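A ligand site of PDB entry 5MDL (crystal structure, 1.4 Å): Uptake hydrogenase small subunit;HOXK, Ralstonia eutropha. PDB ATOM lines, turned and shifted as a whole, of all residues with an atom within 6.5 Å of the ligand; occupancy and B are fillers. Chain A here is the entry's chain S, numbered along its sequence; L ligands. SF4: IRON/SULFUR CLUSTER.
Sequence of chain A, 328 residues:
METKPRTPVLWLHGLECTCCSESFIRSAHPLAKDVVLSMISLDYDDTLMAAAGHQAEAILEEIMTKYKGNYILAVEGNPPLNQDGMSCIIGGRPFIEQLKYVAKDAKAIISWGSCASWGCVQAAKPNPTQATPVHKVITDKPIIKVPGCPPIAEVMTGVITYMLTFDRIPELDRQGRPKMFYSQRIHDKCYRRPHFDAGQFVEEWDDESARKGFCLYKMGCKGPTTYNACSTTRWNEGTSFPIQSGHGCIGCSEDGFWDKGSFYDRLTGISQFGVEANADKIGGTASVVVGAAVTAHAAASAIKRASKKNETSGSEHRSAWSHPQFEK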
ATOM      1  N   ILE A 186      16.788  12.630  22.077  1.00  0.00           N
ATOM      2  CA  ILE A 186      17.918  11.718  22.283  1.00  0.00           C
ATOM      3  C   ILE A 186      19.196  12.528  22.590  1.00  0.00           C
ATOM      4  O   ILE A 186      19.947  12.185  23.475  1.00  0.00           O
ATOM      5  CB  ILE A 186      18.185  10.848  21.019  1.00  0.00           C
ATOM      6  CG1 ILE A 186      16.958  10.063  20.546  1.00  0.00           C
ATOM      7  CG2 ILE A 186      19.329   9.882  21.248  1.00  0.00           C
ATOM      8  CD1 ILE A 186      16.298   9.250  21.618  1.00  0.00           C
ATOM      9  N   HIS A 187      19.373  13.603  21.833  1.00  0.00           N
ATOM     10  CA  HIS A 187      20.566  14.457  21.864  1.00  0.00           C
ATOM     11  C   HIS A 187      20.770  15.195  23.205  1.00  0.00           C
ATOM     12  O   HIS A 187      21.891  15.568  23.530  1.00  0.00           O
ATOM     13  CB  HIS A 187      20.426  15.446  20.691  1.00  0.00           C
ATOM     14  CG  HIS A 187      21.569  16.383  20.484  1.00  0.00           C
ATOM     15  ND1 HIS A 187      22.757  15.994  19.925  1.00  0.00           N
ATOM     16  CD2 HIS A 187      21.653  17.717  20.660  1.00  0.00           C
ATOM     17  CE1 HIS A 187      23.551  17.044  19.812  1.00  0.00           C
ATOM     18  NE2 HIS A 187      22.894  18.110  20.251  1.00  0.00           N
ATOM     19  N   ASP A 188      19.695  15.364  23.995  1.00  0.00           N
ATOM     20  CA  ASP A 188      19.775  16.093  25.274  1.00  0.00           C
ATOM     21  C   ASP A 188      20.778  15.429  26.250  1.00  0.00           C
ATOM     22  O   ASP A 188      21.655  16.096  26.787  1.00  0.00           O
ATOM     23  CB  ASP A 188      18.392  16.189  25.960  1.00  0.00           C
ATOM     24  CG  ASP A 188      17.387  17.068  25.203  1.00  0.00           C
ATOM     25  OD1 ASP A 188      17.801  17.921  24.392  1.00  0.00           O
ATOM     26  OD2 ASP A 188      16.165  16.939  25.460  1.00  0.00           O
ATOM     27  N   CYS A 190      22.379  12.200  25.458  1.00  0.00           N
ATOM     28  CA  CYS A 190      23.276  11.281  24.776  1.00  0.00           C
ATOM     29  C   CYS A 190      24.681  11.393  25.361  1.00  0.00           C
ATOM     30  O   CYS A 190      25.228  12.498  25.416  1.00  0.00           O
ATOM     31  CB  CYS A 190      23.336  11.614  23.290  1.00  0.00           C
ATOM     32  SG  CYS A 190      24.401  10.496  22.357  1.00  0.00           S
ATOM     33  N   TYR A 191      25.272  10.274  25.763  1.00  0.00           N
ATOM     34  CA  TYR A 191      26.618  10.274  26.351  1.00  0.00           C
ATOM     35  C   TYR A 191      27.699  10.783  25.395  1.00  0.00           C
ATOM     36  O   TYR A 191      28.788  11.121  25.864  1.00  0.00           O
ATOM     37  CB  TYR A 191      27.017   8.900  26.905  1.00  0.00           C
ATOM     38  CG  TYR A 191      27.531   7.947  25.852  1.00  0.00           C
ATOM     39  CD1 TYR A 191      26.646   7.307  24.972  1.00  0.00           C
ATOM     40  CD2 TYR A 191      28.884   7.675  25.718  1.00  0.00           C
ATOM     41  CE1 TYR A 191      27.113   6.437  24.008  1.00  0.00           C
ATOM     42  CE2 TYR A 191      29.360   6.809  24.759  1.00  0.00           C
ATOM     43  CZ  TYR A 191      28.461   6.200  23.895  1.00  0.00           C
ATOM     44  OH  TYR A 191      28.914   5.337  22.928  1.00  0.00           O
ATOM     45  N   ARG A 192      27.437  10.811  24.086  1.00  0.00           N
ATOM     46  CA  ARG A 192      28.390  11.370  23.107  1.00  0.00           C
ATOM     47  C   ARG A 192      28.237  12.889  22.907  1.00  0.00           C
ATOM     48  O   ARG A 192      28.959  13.486  22.105  1.00  0.00           O
ATOM     49  CB  ARG A 192      28.247  10.656  21.752  1.00  0.00           C
ATOM     50  CG  ARG A 192      28.514   9.162  21.828  1.00  0.00           C
ATOM     51  CD  ARG A 192      28.686   8.554  20.455  1.00  0.00           C
ATOM     52  NE  ARG A 192      28.861   7.116  20.551  1.00  0.00           N
ATOM     53  CZ  ARG A 192      29.498   6.367  19.647  1.00  0.00           C
ATOM     54  NH1 ARG A 192      30.023   6.899  18.552  1.00  0.00           N
ATOM     55  NH2 ARG A 192      29.607   5.047  19.855  1.00  0.00           N
ATOM     56  N   ARG A 193      27.317  13.510  23.628  1.00  0.00           N
ATOM     57  CA  ARG A 193      27.080  14.956  23.543  1.00  0.00           C
ATOM     58  C   ARG A 193      28.329  15.827  23.783  1.00  0.00           C
ATOM     59  O   ARG A 193      28.551  16.783  23.051  1.00  0.00           O
ATOM     60  CB  ARG A 193      25.906  15.356  24.446  1.00  0.00           C
ATOM     61  CG  ARG A 193      25.517  16.836  24.453  1.00  0.00           C
ATOM     62  CD  ARG A 193      25.061  17.323  23.093  1.00  0.00           C
ATOM     63  NE  ARG A 193      24.747  18.750  23.149  1.00  0.00           N
ATOM     64  CZ  ARG A 193      23.570  19.278  23.468  1.00  0.00           C
ATOM     65  NH1 ARG A 193      22.530  18.513  23.780  1.00  0.00           N
ATOM     66  NH2 ARG A 193      23.435  20.602  23.488  1.00  0.00           N
ATOM     67  N   PRO A 194      29.177  15.484  24.780  1.00  0.00           N
ATOM     68  CA  PRO A 194      30.406  16.267  24.959  1.00  0.00           C
ATOM     69  C   PRO A 194      31.288  16.273  23.708  1.00  0.00           C
ATOM     70  O   PRO A 194      31.863  17.297  23.390  1.00  0.00           O
ATOM     71  CB  PRO A 194      31.097  15.564  26.120  1.00  0.00           C
ATOM     72  CG  PRO A 194      29.951  15.013  26.926  1.00  0.00           C
ATOM     73  CD  PRO A 194      29.002  14.505  25.872  1.00  0.00           C
ATOM     74  N   HIS A 195      31.317  15.160  22.974  1.00  0.00           N
ATOM     75  CA  HIS A 195      32.015  15.141  21.687  1.00  0.00           C
ATOM     76  C   HIS A 195      31.357  16.070  20.657  1.00  0.00           C
ATOM     77  O   HIS A 195      32.047  16.823  19.964  1.00  0.00           O
ATOM     78  CB  HIS A 195      32.145  13.717  21.134  1.00  0.00           C
ATOM     79  CG  HIS A 195      33.039  12.834  21.951  1.00  0.00           C
ATOM     80  ND1 HIS A 195      34.359  13.133  22.203  1.00  0.00           N
ATOM     81  CD2 HIS A 195      32.799  11.644  22.554  1.00  0.00           C
ATOM     82  CE1 HIS A 195      34.895  12.172  22.918  1.00  0.00           C
ATOM     83  NE2 HIS A 195      33.970  11.257  23.148  1.00  0.00           N
ATOM     84  N   PHE A 196      30.032  16.042  20.581  1.00  0.00           N
ATOM     85  CA  PHE A 196      29.310  16.978  19.732  1.00  0.00           C
ATOM     86  C   PHE A 196      29.670  18.412  20.085  1.00  0.00           C
ATOM     87  O   PHE A 196      29.968  19.205  19.202  1.00  0.00           O
ATOM     88  CB  PHE A 196      27.795  16.791  19.848  1.00  0.00           C
ATOM     89  CG  PHE A 196      26.986  17.781  19.053  1.00  0.00           C
ATOM     90  CD1 PHE A 196      26.601  18.996  19.613  1.00  0.00           C
ATOM     91  CD2 PHE A 196      26.585  17.483  17.765  1.00  0.00           C
ATOM     92  CE1 PHE A 196      25.851  19.894  18.884  1.00  0.00           C
ATOM     93  CE2 PHE A 196      25.812  18.385  17.029  1.00  0.00           C
ATOM     94  CZ  PHE A 196      25.449  19.596  17.597  1.00  0.00           C
ATOM     95  N   PHE A 201      33.686  14.392  15.700  1.00  0.00           N
ATOM     96  CA  PHE A 201      32.743  13.609  14.909  1.00  0.00           C
ATOM     97  C   PHE A 201      33.393  12.451  14.184  1.00  0.00           C
ATOM     98  O   PHE A 201      34.526  12.555  13.694  1.00  0.00           O
ATOM     99  CB  PHE A 201      32.095  14.492  13.840  1.00  0.00           C
ATOM    100  CG  PHE A 201      31.366  15.663  14.391  1.00  0.00           C
ATOM    101  CD1 PHE A 201      30.145  15.497  15.033  1.00  0.00           C
ATOM    102  CD2 PHE A 201      31.888  16.958  14.262  1.00  0.00           C
ATOM    103  CE1 PHE A 201      29.454  16.582  15.531  1.00  0.00           C
ATOM    104  CE2 PHE A 201      31.191  18.047  14.768  1.00  0.00           C
ATOM    105  CZ  PHE A 201      29.979  17.861  15.413  1.00  0.00           C
ATOM    106  N   PHE A 214      33.226   8.986  19.179  1.00  0.00           N
ATOM    107  CA  PHE A 214      32.889  10.357  18.820  1.00  0.00           C
ATOM    108  C   PHE A 214      31.435  10.455  18.303  1.00  0.00           C
ATOM    109  O   PHE A 214      30.816   9.443  17.931  1.00  0.00           O
ATOM    110  CB  PHE A 214      33.873  10.914  17.771  1.00  0.00           C
ATOM    111  CG  PHE A 214      35.188  11.409  18.347  1.00  0.00           C
ATOM    112  CD1 PHE A 214      35.603  11.085  19.636  1.00  0.00           C
ATOM    113  CD2 PHE A 214      36.039  12.154  17.544  1.00  0.00           C
ATOM    114  CE1 PHE A 214      36.827  11.553  20.131  1.00  0.00           C
ATOM    115  CE2 PHE A 214      37.256  12.610  18.040  1.00  0.00           C
ATOM    116  CZ  PHE A 214      37.641  12.301  19.323  1.00  0.00           C
ATOM    117  N   CYS A 215      30.915  11.669  18.311  1.00  0.00           N
ATOM    118  CA  CYS A 215      29.531  11.934  17.915  1.00  0.00           C
ATOM    119  C   CYS A 215      29.257  11.446  16.478  1.00  0.00           C
ATOM    120  O   CYS A 215      30.102  11.537  15.590  1.00  0.00           O
ATOM    121  CB  CYS A 215      29.235  13.425  18.054  1.00  0.00           C
ATOM    122  SG  CYS A 215      27.626  13.952  17.408  1.00  0.00           S
ATOM    123  N   LEU A 216      28.042  10.925  16.283  1.00  0.00           N
ATOM    124  CA  LEU A 216      27.605  10.359  15.009  1.00  0.00           C
ATOM    125  C   LEU A 216      26.757  11.312  14.142  1.00  0.00           C
ATOM    126  O   LEU A 216      26.198  10.897  13.126  1.00  0.00           O
ATOM    127  CB  LEU A 216      26.819   9.078  15.282  1.00  0.00           C
ATOM    128  CG  LEU A 216      27.660   7.987  15.943  1.00  0.00           C
ATOM    129  CD1 LEU A 216      26.795   6.867  16.521  1.00  0.00           C
ATOM    130  CD2 LEU A 216      28.638   7.415  14.940  1.00  0.00           C
ATOM    131  N   TYR A 217      26.720  12.602  14.489  1.00  0.00           N
ATOM    132  CA  TYR A 217      25.971  13.610  13.708  1.00  0.00           C
ATOM    133  C   TYR A 217      26.268  13.595  12.214  1.00  0.00           C
ATOM    134  O   TYR A 217      25.360  13.615  11.377  1.00  0.00           O
ATOM    135  CB  TYR A 217      26.252  15.018  14.231  1.00  0.00           C
ATOM    136  CG  TYR A 217      25.378  16.120  13.635  1.00  0.00           C
ATOM    137  CD1 TYR A 217      24.152  16.450  14.203  1.00  0.00           C
ATOM    138  CD2 TYR A 217      25.792  16.838  12.523  1.00  0.00           C
ATOM    139  CE1 TYR A 217      23.360  17.472  13.688  1.00  0.00           C
ATOM    140  CE2 TYR A 217      25.011  17.861  11.989  1.00  0.00           C
ATOM    141  CZ  TYR A 217      23.796  18.169  12.577  1.00  0.00           C
ATOM    142  OH  TYR A 217      23.038  19.189  12.050  1.00  0.00           O
ATOM    143  N   LYS A 218      27.548  13.579  11.879  1.00  0.00           N
ATOM    144  CA  LYS A 218      27.942  13.628  10.466  1.00  0.00           C
ATOM    145  C   LYS A 218      27.750  12.303   9.728  1.00  0.00           C
ATOM    146  O   LYS A 218      27.834  12.264   8.497  1.00  0.00           O
ATOM    147  CB  LYS A 218      29.386  14.124  10.352  1.00  0.00           C
ATOM    148  CG  LYS A 218      29.531  15.561  10.800  1.00  0.00           C
ATOM    149  CD  LYS A 218      30.953  16.090  10.650  1.00  0.00           C
ATOM    150  CE  LYS A 218      30.999  17.582  10.901  1.00  0.00           C
ATOM    151  NZ  LYS A 218      32.375  18.142  10.696  1.00  0.00           N
ATOM    152  N   CYS A 221      23.112  10.873  12.298  1.00  0.00           N
ATOM    153  CA  CYS A 221      22.358  10.704  13.541  1.00  0.00           C
ATOM    154  C   CYS A 221      21.219  11.725  13.613  1.00  0.00           C
ATOM    155  O   CYS A 221      21.426  12.930  13.509  1.00  0.00           O
ATOM    156  CB  CYS A 221      23.265  10.848  14.763  1.00  0.00           C
ATOM    157  SG  CYS A 221      22.391  10.551  16.330  1.00  0.00           S
ATOM    158  N   LYS A 222      20.004  11.232  13.812  1.00  0.00           N
ATOM    159  CA  LYS A 222      18.823  12.060  13.927  1.00  0.00           C
ATOM    160  C   LYS A 222      18.396  12.285  15.391  1.00  0.00           C
ATOM    161  O   LYS A 222      17.293  12.773  15.665  1.00  0.00           O
ATOM    162  CB  LYS A 222      17.681  11.452  13.104  1.00  0.00           C
ATOM    163  CG  LYS A 222      17.975  11.327  11.604  1.00  0.00           C
ATOM    164  CD  LYS A 222      18.602  12.611  11.023  1.00  0.00           C
ATOM    165  CE  LYS A 222      18.701  12.611   9.505  1.00  0.00           C
ATOM    166  NZ  LYS A 222      19.411  11.419   8.962  1.00  0.00           N
ATOM    167  N   GLY A 223      19.293  11.963  16.334  1.00  0.00           N
ATOM    168  CA  GLY A 223      19.070  12.231  17.743  1.00  0.00           C
ATOM    169  C   GLY A 223      18.652  13.657  18.075  1.00  0.00           C
ATOM    170  O   GLY A 223      17.821  13.861  18.961  1.00  0.00           O
ATOM    171  N   PRO A 224      19.206  14.664  17.367  1.00  0.00           N
ATOM    172  CA  PRO A 224      18.793  16.052  17.637  1.00  0.00           C
ATOM    173  C   PRO A 224      17.333  16.408  17.371  1.00  0.00           C
ATOM    174  O   PRO A 224      16.873  17.414  17.896  1.00  0.00           O
ATOM    175  CB  PRO A 224      19.733  16.884  16.742  1.00  0.00           C
ATOM    176  CG  PRO A 224      20.947  16.038  16.609  1.00  0.00           C
ATOM    177  CD  PRO A 224      20.417  14.613  16.525  1.00  0.00           C
ATOM    178  N   SER A 231      18.512   7.440  25.288  1.00  0.00           N
ATOM    179  CA  SER A 231      19.813   7.862  25.844  1.00  0.00           C
ATOM    180  C   SER A 231      19.914   7.644  27.345  1.00  0.00           C
ATOM    181  O   SER A 231      20.999   7.540  27.883  1.00  0.00           O
ATOM    182  CB  SER A 231      20.072   9.345  25.525  1.00  0.00           C
ATOM    183  OG  SER A 231      20.265   9.524  24.142  1.00  0.00           O
ATOM    184  N   PHE A 241      22.150   1.335  23.405  1.00  0.00           N
ATOM    185  CA  PHE A 241      21.172   1.941  22.521  1.00  0.00           C
ATOM    186  C   PHE A 241      21.871   2.159  21.179  1.00  0.00           C
ATOM    187  O   PHE A 241      23.084   1.946  21.078  1.00  0.00           O
ATOM    188  CB  PHE A 241      20.519   3.201  23.124  1.00  0.00           C
ATOM    189  CG  PHE A 241      21.403   4.417  23.205  1.00  0.00           C
ATOM    190  CD1 PHE A 241      22.487   4.475  24.087  1.00  0.00           C
ATOM    191  CD2 PHE A 241      21.024   5.586  22.541  1.00  0.00           C
ATOM    192  CE1 PHE A 241      23.219   5.653  24.239  1.00  0.00           C
ATOM    193  CE2 PHE A 241      21.762   6.760  22.686  1.00  0.00           C
ATOM    194  CZ  PHE A 241      22.863   6.784  23.528  1.00  0.00           C
ATOM    195  N   ILE A 243      23.113   4.507  19.367  1.00  0.00           N
ATOM    196  CA  ILE A 243      24.316   5.355  19.366  1.00  0.00           C
ATOM    197  C   ILE A 243      25.466   4.713  20.148  1.00  0.00           C
ATOM    198  O   ILE A 243      26.610   4.707  19.650  1.00  0.00           O
ATOM    199  CB  ILE A 243      23.951   6.758  19.881  1.00  0.00           C
ATOM    200  CG1 ILE A 243      23.122   7.479  18.804  1.00  0.00           C
ATOM    201  CG2 ILE A 243      25.167   7.579  20.300  1.00  0.00           C
ATOM    202  CD1 ILE A 243      22.135   8.496  19.319  1.00  0.00           C
ATOM    203  N   GLY A 248      24.066   5.919  14.181  1.00  0.00           N
ATOM    204  CA  GLY A 248      23.242   7.078  14.501  1.00  0.00           C
ATOM    205  C   GLY A 248      21.798   6.657  14.720  1.00  0.00           C
ATOM    206  O   GLY A 248      21.315   5.680  14.139  1.00  0.00           O
ATOM    207  N   CYS A 249      21.097   7.406  15.540  1.00  0.00           N
ATOM    208  CA  CYS A 249      19.649   7.334  15.575  1.00  0.00           C
ATOM    209  C   CYS A 249      19.128   7.557  14.146  1.00  0.00           C
ATOM    210  O   CYS A 249      19.607   8.467  13.433  1.00  0.00           O
ATOM    211  CB  CYS A 249      19.128   8.416  16.532  1.00  0.00           C
ATOM    212  SG  CYS A 249      17.352   8.589  16.643  1.00  0.00           S
HETATM  213 FE1  SF4 L   1      23.558  11.789  17.855  1.00  0.00          FE
HETATM  214 FE2  SF4 L   1      25.864  13.093  18.534  1.00  0.00          FE
HETATM  215 FE3  SF4 L   1      24.464  11.749  20.445  1.00  0.00          FE
HETATM  216 FE4  SF4 L   1      23.522  14.126  19.403  1.00  0.00          FE
HETATM  217  S1  SF4 L   1      25.442  13.797  20.630  1.00  0.00           S
HETATM  218  S2  SF4 L   1      22.322  12.162  19.758  1.00  0.00           S
HETATM  219  S3  SF4 L   1      24.137  13.885  17.167  1.00  0.00           S
HETATM  220  S4  SF4 L   1      25.542  10.854  18.614  1.00  0.00           S
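The backbone NH (N) of Arg 193 lies close to a sulfur (S1) of the ligand. FE3 of the ligand is bound by SG of Cys 190, at 2.3 Å. ND1 of His 187 is bound to FE4 of the ligand (2.1 Å). SG of Cys 221 binds FE1 of the ligand. The side-chain sulfur (SG) of Cys 215 is bound to an iron atom (FE2) of the ligand (2.3 Å). N of Leu 216 lies close to S4 of the ligand (3.4 Å).
O of His 187 is in hydrogen-bond range of NH1 of Arg 193, at 3.0 Å. The side-chain sulfur of Cys 221 sits close to the backbone NH of Gly 223, 3.4 Å away. The guanidinium group (NH1) of Arg 192 sits at hydrogen-bond distance from the backbone carbonyl oxygen (O) of Phe 214. The side-chain sulfur of Cys 190 lies close to the backbone NH of Arg 192, 3.5 Å away. N of Cys 249 lies close to SG of Cys 221 (3.5 Å). O of Ile 243 sits at hydrogen-bond distance from NH2 of Arg 192. O of Leu 216 is in hydrogen-bond range of N of Cys 221 (3.2 Å). OH of Tyr 191 is in hydrogen-bond range of NE of Arg 192, at 3.0 Å.
Merely in contact with the ligand: Ile 243 (3.7 Å), Arg 192 (3.7 Å), Tyr 217 (3.8 Å), Gly 223 (3.8 Å), Pro 224 (3.8 Å) and Phe 196 (3.9 Å). Hydrophobic or aromatic side chains that line the ligand: His 187, Phe 196, Leu 216, Tyr 217, Pro 224 and Ile 243. Within 4 Å of the ligand: His 187, Cys 190, Arg 192, Arg 193, Phe 196, Cys 215, Leu 216, Tyr 217, Cys 221, Gly 223, Pro 224 and Ile 243.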
